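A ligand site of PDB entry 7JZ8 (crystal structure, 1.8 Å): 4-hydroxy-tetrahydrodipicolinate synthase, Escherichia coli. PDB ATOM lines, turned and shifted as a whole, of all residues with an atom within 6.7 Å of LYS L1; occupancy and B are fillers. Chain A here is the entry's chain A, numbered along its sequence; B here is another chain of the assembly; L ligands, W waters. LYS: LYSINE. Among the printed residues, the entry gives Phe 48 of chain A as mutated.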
ATOM      1  N   VAL A  42     -17.628  16.089 -24.007  1.00  0.00           N
ATOM      2  CA  VAL A  42     -19.087  16.195 -23.760  1.00  0.00           C
ATOM      3  C   VAL A  42     -19.477  15.240 -22.603  1.00  0.00           C
ATOM      4  O   VAL A  42     -20.385  14.442 -22.729  1.00  0.00           O
ATOM      5  CB  VAL A  42     -19.942  15.958 -25.018  1.00  0.00           C
ATOM      6  CG1 VAL A  42     -21.360  16.453 -24.739  1.00  0.00           C
ATOM      7  CG2 VAL A  42     -19.427  16.727 -26.242  1.00  0.00           C
ATOM      8  N   GLU A  47     -21.343  19.903 -20.767  1.00  0.00           N
ATOM      9  CA  GLU A  47     -22.723  20.243 -21.035  1.00  0.00           C
ATOM     10  C   GLU A  47     -23.488  19.203 -21.847  1.00  0.00           C
ATOM     11  O   GLU A  47     -24.359  19.527 -22.679  1.00  0.00           O
ATOM     12  CB  GLU A  47     -22.918  21.657 -21.552  1.00  0.00           C
ATOM     13  CG  GLU A  47     -22.791  22.683 -20.397  1.00  0.00           C
ATOM     14  CD  GLU A  47     -22.675  24.107 -20.919  1.00  0.00           C
ATOM     15  OE1 GLU A  47     -21.510  24.543 -21.281  1.00  0.00           O
ATOM     16  OE2 GLU A  47     -23.734  24.796 -20.980  1.00  0.00           O
ATOM     17  N   PHE A  48     -23.211  17.971 -21.571  1.00  0.00           N
ATOM     18  CA  PHE A  48     -24.014  16.938 -22.195  1.00  0.00           C
ATOM     19  C   PHE A  48     -25.480  17.050 -22.096  1.00  0.00           C
ATOM     20  O   PHE A  48     -26.173  16.735 -23.059  1.00  0.00           O
ATOM     21  CB  PHE A  48     -23.521  15.520 -21.945  1.00  0.00           C
ATOM     22  CG  PHE A  48     -24.184  14.757 -20.834  1.00  0.00           C
ATOM     23  CD1 PHE A  48     -25.464  14.290 -20.929  1.00  0.00           C
ATOM     24  CD2 PHE A  48     -23.462  14.501 -19.666  1.00  0.00           C
ATOM     25  CE1 PHE A  48     -26.070  13.597 -19.915  1.00  0.00           C
ATOM     26  CE2 PHE A  48     -24.023  13.795 -18.607  1.00  0.00           C
ATOM     27  CZ  PHE A  48     -25.350  13.337 -18.730  1.00  0.00           C
ATOM     28  N   ALA A  49     -25.961  17.565 -20.995  1.00  0.00           N
ATOM     29  CA  ALA A  49     -27.430  17.650 -20.831  1.00  0.00           C
ATOM     30  C   ALA A  49     -28.105  18.630 -21.791  1.00  0.00           C
ATOM     31  O   ALA A  49     -29.260  18.437 -22.203  1.00  0.00           O
ATOM     32  CB  ALA A  49     -27.701  18.092 -19.397  1.00  0.00           C
ATOM     33  N   THR A  50     -27.376  19.649 -22.211  1.00  0.00           N
ATOM     34  CA  THR A  50     -28.032  20.651 -23.027  1.00  0.00           C
ATOM     35  C   THR A  50     -27.645  20.684 -24.531  1.00  0.00           C
ATOM     36  O   THR A  50     -28.095  21.602 -25.232  1.00  0.00           O
ATOM     37  CB  THR A  50     -27.813  22.043 -22.440  1.00  0.00           C
ATOM     38  OG1 THR A  50     -26.449  22.338 -22.319  1.00  0.00           O
ATOM     39  CG2 THR A  50     -28.468  22.147 -21.059  1.00  0.00           C
ATOM     40  N   LEU A  51     -26.840  19.734 -24.942  1.00  0.00           N
ATOM     41  CA  LEU A  51     -26.607  19.515 -26.415  1.00  0.00           C
ATOM     42  C   LEU A  51     -27.516  18.434 -26.830  1.00  0.00           C
ATOM     43  O   LEU A  51     -27.653  17.451 -26.130  1.00  0.00           O
ATOM     44  CB  LEU A  51     -25.186  19.091 -26.601  1.00  0.00           C
ATOM     45  CG  LEU A  51     -24.141  20.058 -26.151  1.00  0.00           C
ATOM     46  CD1 LEU A  51     -22.734  19.498 -26.434  1.00  0.00           C
ATOM     47  CD2 LEU A  51     -24.250  21.388 -26.747  1.00  0.00           C
ATOM     48  N   ASN A  52     -28.055  18.562 -28.034  1.00  0.00           N
ATOM     49  CA  ASN A  52     -28.807  17.435 -28.672  1.00  0.00           C
ATOM     50  C   ASN A  52     -27.843  16.409 -29.162  1.00  0.00           C
ATOM     51  O   ASN A  52     -26.618  16.646 -29.120  1.00  0.00           O
ATOM     52  CB  ASN A  52     -29.871  17.922 -29.689  1.00  0.00           C
ATOM     53  CG  ASN A  52     -29.277  18.482 -30.902  1.00  0.00           C
ATOM     54  OD1 ASN A  52     -28.282  17.937 -31.383  1.00  0.00           O
ATOM     55  ND2 ASN A  52     -29.863  19.586 -31.430  1.00  0.00           N
ATOM     56  N   HIS A  53     -28.295  15.231 -29.559  1.00  0.00           N
ATOM     57  CA  HIS A  53     -27.358  14.161 -29.902  1.00  0.00           C
ATOM     58  C   HIS A  53     -26.499  14.553 -31.093  1.00  0.00           C
ATOM     59  O   HIS A  53     -25.350  14.195 -31.174  1.00  0.00           O
ATOM     60  CB  HIS A  53     -28.030  12.832 -30.294  1.00  0.00           C
ATOM     61  CG  HIS A  53     -28.263  11.915 -29.126  1.00  0.00           C
ATOM     62  ND1 HIS A  53     -28.605  10.590 -29.261  1.00  0.00           N
ATOM     63  CD2 HIS A  53     -28.213  12.163 -27.790  1.00  0.00           C
ATOM     64  CE1 HIS A  53     -28.783  10.060 -28.060  1.00  0.00           C
ATOM     65  NE2 HIS A  53     -28.536  10.984 -27.150  1.00  0.00           N
ATOM     66  N   ASP A  54     -27.070  15.264 -32.040  1.00  0.00           N
ATOM     67  CA  ASP A  54     -26.231  15.688 -33.191  1.00  0.00           C
ATOM     68  C   ASP A  54     -25.184  16.669 -32.816  1.00  0.00           C
ATOM     69  O   ASP A  54     -24.030  16.608 -33.272  1.00  0.00           O
ATOM     70  CB  ASP A  54     -27.158  16.253 -34.300  1.00  0.00           C
ATOM     71  CG  ASP A  54     -27.955  15.185 -34.978  1.00  0.00           C
ATOM     72  OD1 ASP A  54     -27.478  14.068 -35.265  1.00  0.00           O
ATOM     73  OD2 ASP A  54     -29.119  15.431 -35.180  1.00  0.00           O
ATOM     74  N   HIS A  56     -23.902  17.042 -29.899  1.00  0.00           N
ATOM     75  CA  HIS A  56     -22.985  16.297 -29.023  1.00  0.00           C
ATOM     76  C   HIS A  56     -21.953  15.581 -29.907  1.00  0.00           C
ATOM     77  O   HIS A  56     -20.698  15.697 -29.714  1.00  0.00           O
ATOM     78  CB  HIS A  56     -23.853  15.331 -28.245  1.00  0.00           C
ATOM     79  CG  HIS A  56     -23.128  14.426 -27.292  1.00  0.00           C
ATOM     80  ND1 HIS A  56     -23.764  13.980 -26.119  1.00  0.00           N
ATOM     81  CD2 HIS A  56     -21.943  13.779 -27.360  1.00  0.00           C
ATOM     82  CE1 HIS A  56     -22.962  13.146 -25.492  1.00  0.00           C
ATOM     83  NE2 HIS A  56     -21.830  13.033 -26.194  1.00  0.00           N
ATOM     84  N   ALA A  57     -22.471  14.892 -30.889  1.00  0.00           N
ATOM     85  CA  ALA A  57     -21.590  14.165 -31.795  1.00  0.00           C
ATOM     86  C   ALA A  57     -20.667  15.122 -32.567  1.00  0.00           C
ATOM     87  O   ALA A  57     -19.471  14.809 -32.757  1.00  0.00           O
ATOM     88  CB  ALA A  57     -22.405  13.246 -32.711  1.00  0.00           C
ATOM     89  N   GLY A  78     -23.296   8.596 -22.150  1.00  0.00           N
ATOM     90  CA  GLY A  78     -24.388   8.147 -21.269  1.00  0.00           C
ATOM     91  C   GLY A  78     -25.759   8.613 -21.711  1.00  0.00           C
ATOM     92  O   GLY A  78     -25.942   9.569 -22.506  1.00  0.00           O
ATOM     93  N   ALA A  79     -26.757   7.880 -21.209  1.00  0.00           N
ATOM     94  CA  ALA A  79     -28.179   8.235 -21.384  1.00  0.00           C
ATOM     95  C   ALA A  79     -28.965   7.528 -20.307  1.00  0.00           C
ATOM     96  O   ALA A  79     -28.534   6.486 -19.785  1.00  0.00           O
ATOM     97  CB  ALA A  79     -28.727   7.923 -22.751  1.00  0.00           C
ATOM     98  N   ASN A  80     -30.140   8.035 -19.982  1.00  0.00           N
ATOM     99  CA  ASN A  80     -30.954   7.321 -19.017  1.00  0.00           C
ATOM    100  C   ASN A  80     -31.887   6.367 -19.645  1.00  0.00           C
ATOM    101  O   ASN A  80     -32.653   5.742 -18.953  1.00  0.00           O
ATOM    102  CB  ASN A  80     -31.698   8.285 -18.052  1.00  0.00           C
ATOM    103  CG  ASN A  80     -32.646   9.231 -18.775  1.00  0.00           C
ATOM    104  OD1 ASN A  80     -32.765   9.179 -20.018  1.00  0.00           O
ATOM    105  ND2 ASN A  80     -33.426  10.014 -18.005  1.00  0.00           N
ATOM    106  N   GLU A  84     -31.199   4.752 -26.125  1.00  0.00           N
ATOM    107  CA  GLU A  84     -30.590   6.000 -26.450  1.00  0.00           C
ATOM    108  C   GLU A  84     -29.073   5.955 -26.193  1.00  0.00           C
ATOM    109  O   GLU A  84     -28.296   6.457 -26.995  1.00  0.00           O
ATOM    110  CB  GLU A  84     -31.313   7.098 -25.632  1.00  0.00           C
ATOM    111  CG  GLU A  84     -30.817   8.485 -25.726  1.00  0.00           C
ATOM    112  CD  GLU A  84     -31.491   9.494 -24.671  1.00  0.00           C
ATOM    113  OE1 GLU A  84     -32.634   9.179 -24.161  1.00  0.00           O
ATOM    114  OE2 GLU A  84     -30.829  10.564 -24.326  1.00  0.00           O
ATOM    115  N   LEU A  88     -26.244   6.518 -29.180  1.00  0.00           N
ATOM    116  CA  LEU A  88     -25.144   7.416 -29.061  1.00  0.00           C
ATOM    117  C   LEU A  88     -23.794   6.777 -29.190  1.00  0.00           C
ATOM    118  O   LEU A  88     -22.915   7.276 -29.920  1.00  0.00           O
ATOM    119  CB  LEU A  88     -25.276   8.273 -27.833  1.00  0.00           C
ATOM    120  CG  LEU A  88     -24.372   9.377 -27.473  1.00  0.00           C
ATOM    121  CD1 LEU A  88     -24.346  10.486 -28.541  1.00  0.00           C
ATOM    122  CD2 LEU A  88     -24.900  10.001 -26.127  1.00  0.00           C
ATOM    123  N   TYR A 106     -29.974   8.473 -15.042  1.00  0.00           N
ATOM    124  CA  TYR A 106     -30.415   9.528 -14.162  1.00  0.00           C
ATOM    125  C   TYR A 106     -31.921   9.665 -14.212  1.00  0.00           C
ATOM    126  O   TYR A 106     -32.551   9.377 -15.185  1.00  0.00           O
ATOM    127  CB  TYR A 106     -29.747  10.881 -14.468  1.00  0.00           C
ATOM    128  CG  TYR A 106     -29.590  11.108 -15.935  1.00  0.00           C
ATOM    129  CD1 TYR A 106     -30.599  11.757 -16.690  1.00  0.00           C
ATOM    130  CD2 TYR A 106     -28.429  10.676 -16.597  1.00  0.00           C
ATOM    131  CE1 TYR A 106     -30.458  11.928 -18.088  1.00  0.00           C
ATOM    132  CE2 TYR A 106     -28.321  10.830 -17.974  1.00  0.00           C
ATOM    133  CZ  TYR A 106     -29.307  11.461 -18.705  1.00  0.00           C
ATOM    134  OH  TYR A 106     -29.178  11.608 -20.086  1.00  0.00           O
ATOM    135  N   ALA B  79     -38.000  18.832 -19.190  1.00  0.00           N
ATOM    136  CA  ALA B  79     -36.662  18.448 -19.723  1.00  0.00           C
ATOM    137  C   ALA B  79     -35.631  19.097 -18.929  1.00  0.00           C
ATOM    138  O   ALA B  79     -35.866  20.140 -18.269  1.00  0.00           O
ATOM    139  CB  ALA B  79     -36.513  18.888 -21.186  1.00  0.00           C
ATOM    140  N   ASN B  80     -34.434  18.556 -19.002  1.00  0.00           N
ATOM    141  CA  ASN B  80     -33.316  19.172 -18.353  1.00  0.00           C
ATOM    142  C   ASN B  80     -32.559  20.223 -19.167  1.00  0.00           C
ATOM    143  O   ASN B  80     -31.620  20.852 -18.657  1.00  0.00           O
ATOM    144  CB  ASN B  80     -32.345  18.126 -17.757  1.00  0.00           C
ATOM    145  CG  ASN B  80     -31.654  17.286 -18.766  1.00  0.00           C
ATOM    146  OD1 ASN B  80     -31.946  17.327 -19.920  1.00  0.00           O
ATOM    147  ND2 ASN B  80     -30.709  16.445 -18.300  1.00  0.00           N
ATOM    148  N   ALA B  81     -33.000  20.455 -20.388  1.00  0.00           N
ATOM    149  CA  ALA B  81     -32.481  21.542 -21.207  1.00  0.00           C
ATOM    150  C   ALA B  81     -33.644  22.451 -21.537  1.00  0.00           C
ATOM    151  O   ALA B  81     -34.676  21.948 -21.971  1.00  0.00           O
ATOM    152  CB  ALA B  81     -31.876  20.973 -22.513  1.00  0.00           C
ATOM    153  N   GLU B  84     -35.215  22.190 -25.026  1.00  0.00           N
ATOM    154  CA  GLU B  84     -35.915  20.954 -25.259  1.00  0.00           C
ATOM    155  C   GLU B  84     -37.293  20.985 -24.612  1.00  0.00           C
ATOM    156  O   GLU B  84     -38.262  20.493 -25.179  1.00  0.00           O
ATOM    157  CB  GLU B  84     -35.007  19.875 -24.666  1.00  0.00           C
ATOM    158  CG  GLU B  84     -35.400  18.501 -24.812  1.00  0.00           C
ATOM    159  CD  GLU B  84     -34.392  17.445 -24.165  1.00  0.00           C
ATOM    160  OE1 GLU B  84     -33.142  17.778 -23.901  1.00  0.00           O
ATOM    161  OE2 GLU B  84     -34.969  16.313 -23.811  1.00  0.00           O
ATOM    162  N   TYR B 106     -33.055  17.769 -14.244  1.00  0.00           N
ATOM    163  CA  TYR B 106     -32.368  16.641 -13.613  1.00  0.00           C
ATOM    164  C   TYR B 106     -30.936  16.532 -14.127  1.00  0.00           C
ATOM    165  O   TYR B 106     -30.658  16.967 -15.264  1.00  0.00           O
ATOM    166  CB  TYR B 106     -33.140  15.322 -13.843  1.00  0.00           C
ATOM    167  CG  TYR B 106     -33.710  15.179 -15.211  1.00  0.00           C
ATOM    168  CD1 TYR B 106     -33.012  14.590 -16.223  1.00  0.00           C
ATOM    169  CD2 TYR B 106     -34.961  15.680 -15.481  1.00  0.00           C
ATOM    170  CE1 TYR B 106     -33.544  14.478 -17.550  1.00  0.00           C
ATOM    171  CE2 TYR B 106     -35.465  15.600 -16.744  1.00  0.00           C
ATOM    172  CZ  TYR B 106     -34.741  14.991 -17.763  1.00  0.00           C
ATOM    173  OH  TYR B 106     -35.393  14.965 -18.967  1.00  0.00           O
ATOM    174  N   TYR B 107     -30.032  16.078 -13.271  1.00  0.00           N
ATOM    175  CA  TYR B 107     -28.672  15.730 -13.596  1.00  0.00           C
ATOM    176  C   TYR B 107     -27.783  16.974 -13.600  1.00  0.00           C
ATOM    177  O   TYR B 107     -26.723  16.961 -12.931  1.00  0.00           O
ATOM    178  CB  TYR B 107     -28.570  14.933 -14.934  1.00  0.00           C
ATOM    179  CG  TYR B 107     -27.162  14.530 -15.182  1.00  0.00           C
ATOM    180  CD1 TYR B 107     -26.708  13.406 -14.580  1.00  0.00           C
ATOM    181  CD2 TYR B 107     -26.249  15.384 -15.782  1.00  0.00           C
ATOM    182  CE1 TYR B 107     -25.430  12.989 -14.687  1.00  0.00           C
ATOM    183  CE2 TYR B 107     -24.902  15.000 -15.879  1.00  0.00           C
ATOM    184  CZ  TYR B 107     -24.521  13.767 -15.310  1.00  0.00           C
ATOM    185  OH  TYR B 107     -23.230  13.247 -15.283  1.00  0.00           O
HETATM  186  N   LYS L   1     -31.151  16.673 -22.365  1.00  0.00           N
HETATM  187  CA  LYS L   1     -31.426  15.145 -22.423  1.00  0.00           C
HETATM  188  C   LYS L   1     -30.690  14.292 -21.337  1.00  0.00           C
HETATM  189  O   LYS L   1     -29.868  14.800 -20.481  1.00  0.00           O
HETATM  190  CB  LYS L   1     -30.863  14.593 -23.790  1.00  0.00           C
HETATM  191  CG  LYS L   1     -29.364  14.913 -23.997  1.00  0.00           C
HETATM  192  CD  LYS L   1     -28.846  14.234 -25.267  1.00  0.00           C
HETATM  193  CE  LYS L   1     -27.405  13.769 -25.030  1.00  0.00           C
HETATM  194  NZ  LYS L   1     -26.400  14.736 -25.492  1.00  0.00           N
HETATM  195  OXT LYS L   1     -30.762  13.010 -21.362  1.00  0.00           O
HETATM  196  N   LYS L   2     -34.211  10.014 -22.128  1.00  0.00           N
HETATM  197  CA  LYS L   2     -33.977  11.564 -22.118  1.00  0.00           C
HETATM  198  C   LYS L   2     -34.352  12.314 -20.791  1.00  0.00           C
HETATM  199  O   LYS L   2     -34.246  13.582 -20.782  1.00  0.00           O
HETATM  200  CB  LYS L   2     -34.824  12.227 -23.296  1.00  0.00           C
HETATM  201  CG  LYS L   2     -36.344  11.877 -23.145  1.00  0.00           C
HETATM  202  CD  LYS L   2     -37.266  12.670 -24.042  1.00  0.00           C
HETATM  203  CE  LYS L   2     -38.612  12.999 -23.349  1.00  0.00           C
HETATM  204  NZ  LYS L   2     -39.639  11.959 -23.508  1.00  0.00           N
HETATM  205  OXT LYS L   2     -34.875  11.724 -19.779  1.00  0.00           O
HETATM  206  O   HOH W   1     -27.819  11.055 -23.968  1.00  0.00           O
HETATM  207  O   HOH W   2     -30.902  18.499 -25.260  1.00  0.00           O
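The backbone carbonyl oxygen (O) of Tyr 106 of chain B sits at hydrogen-bond distance from the side-chain amide nitrogen (ND2) of Asn 80 of chain B, 3.1 Å away.
The side-chain amide nitrogen (ND2) of Asn 80 of chain A is in hydrogen-bond range of the backbone carbonyl oxygen (O) of Tyr 106 of chain A.
His 53 touches LYS L1 (CD2 to CE, 3.3 Å).
OE2 of Glu 84 of chain A touches OXT of LYS L1, 3.8 Å away.
Hydrophobic or aromatic side chains within 4 Å of LYS L1: His 53, His 56 and Tyr 106 of chain A.
Of the 23 residues printed, 9 come within 4 Å of LYS L1.
Along chain A the residues within 4 Å of LYS L1 span positions 48 to 106.
A nitrogen (N) of LYS L2 is in salt-bridge range of the side-chain carboxylate (OE1) of Glu 84 of chain A (2.7 Å).
A nitrogen (NZ) of LYS L1 sits at hydrogen-bond distance from the backbone carbonyl oxygen of Phe 48, at 3.2 Å.
A ring nitrogen (ND1) of His 56 is in hydrogen-bond range of a nitrogen (NZ) of LYS L1.
A nitrogen (N) of LYS L1 is in salt-bridge range of the side-chain carboxylate (OE1) of Glu 84 of chain B (2.7 Å).
N of LYS L1 lies within hydrogen-bond range of OD1 of Asn 80 of chain B (2.7 Å).
A nitrogen (NZ) of LYS L1 sits at hydrogen-bond distance from the backbone carbonyl oxygen of Leu 51.
OXT of LYS L1 is in hydrogen-bond range of OH of Tyr 106 of chain A (2.5 Å).
O of LYS L2 sits at hydrogen-bond distance from OH of Tyr 106 of chain B, 2.6 Å away.
N of LYS L1 sits at hydrogen-bond distance from O of Ala 49, 2.6 Å away.
The side-chain amide oxygen of Asn 80 of chain A sits at hydrogen-bond distance from a nitrogen (N) of LYS L2.
Water W1 lies within hydrogen-bond range of the backbone carbonyl oxygen of Gly 78, the side-chain carboxylate of Glu 84 of chain A and a ring nitrogen (NE2) of His 53.
Water W2 lies within hydrogen-bond range of OE1 of Glu 84 of chain B, N of LYS L1 and O of Ala 49.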
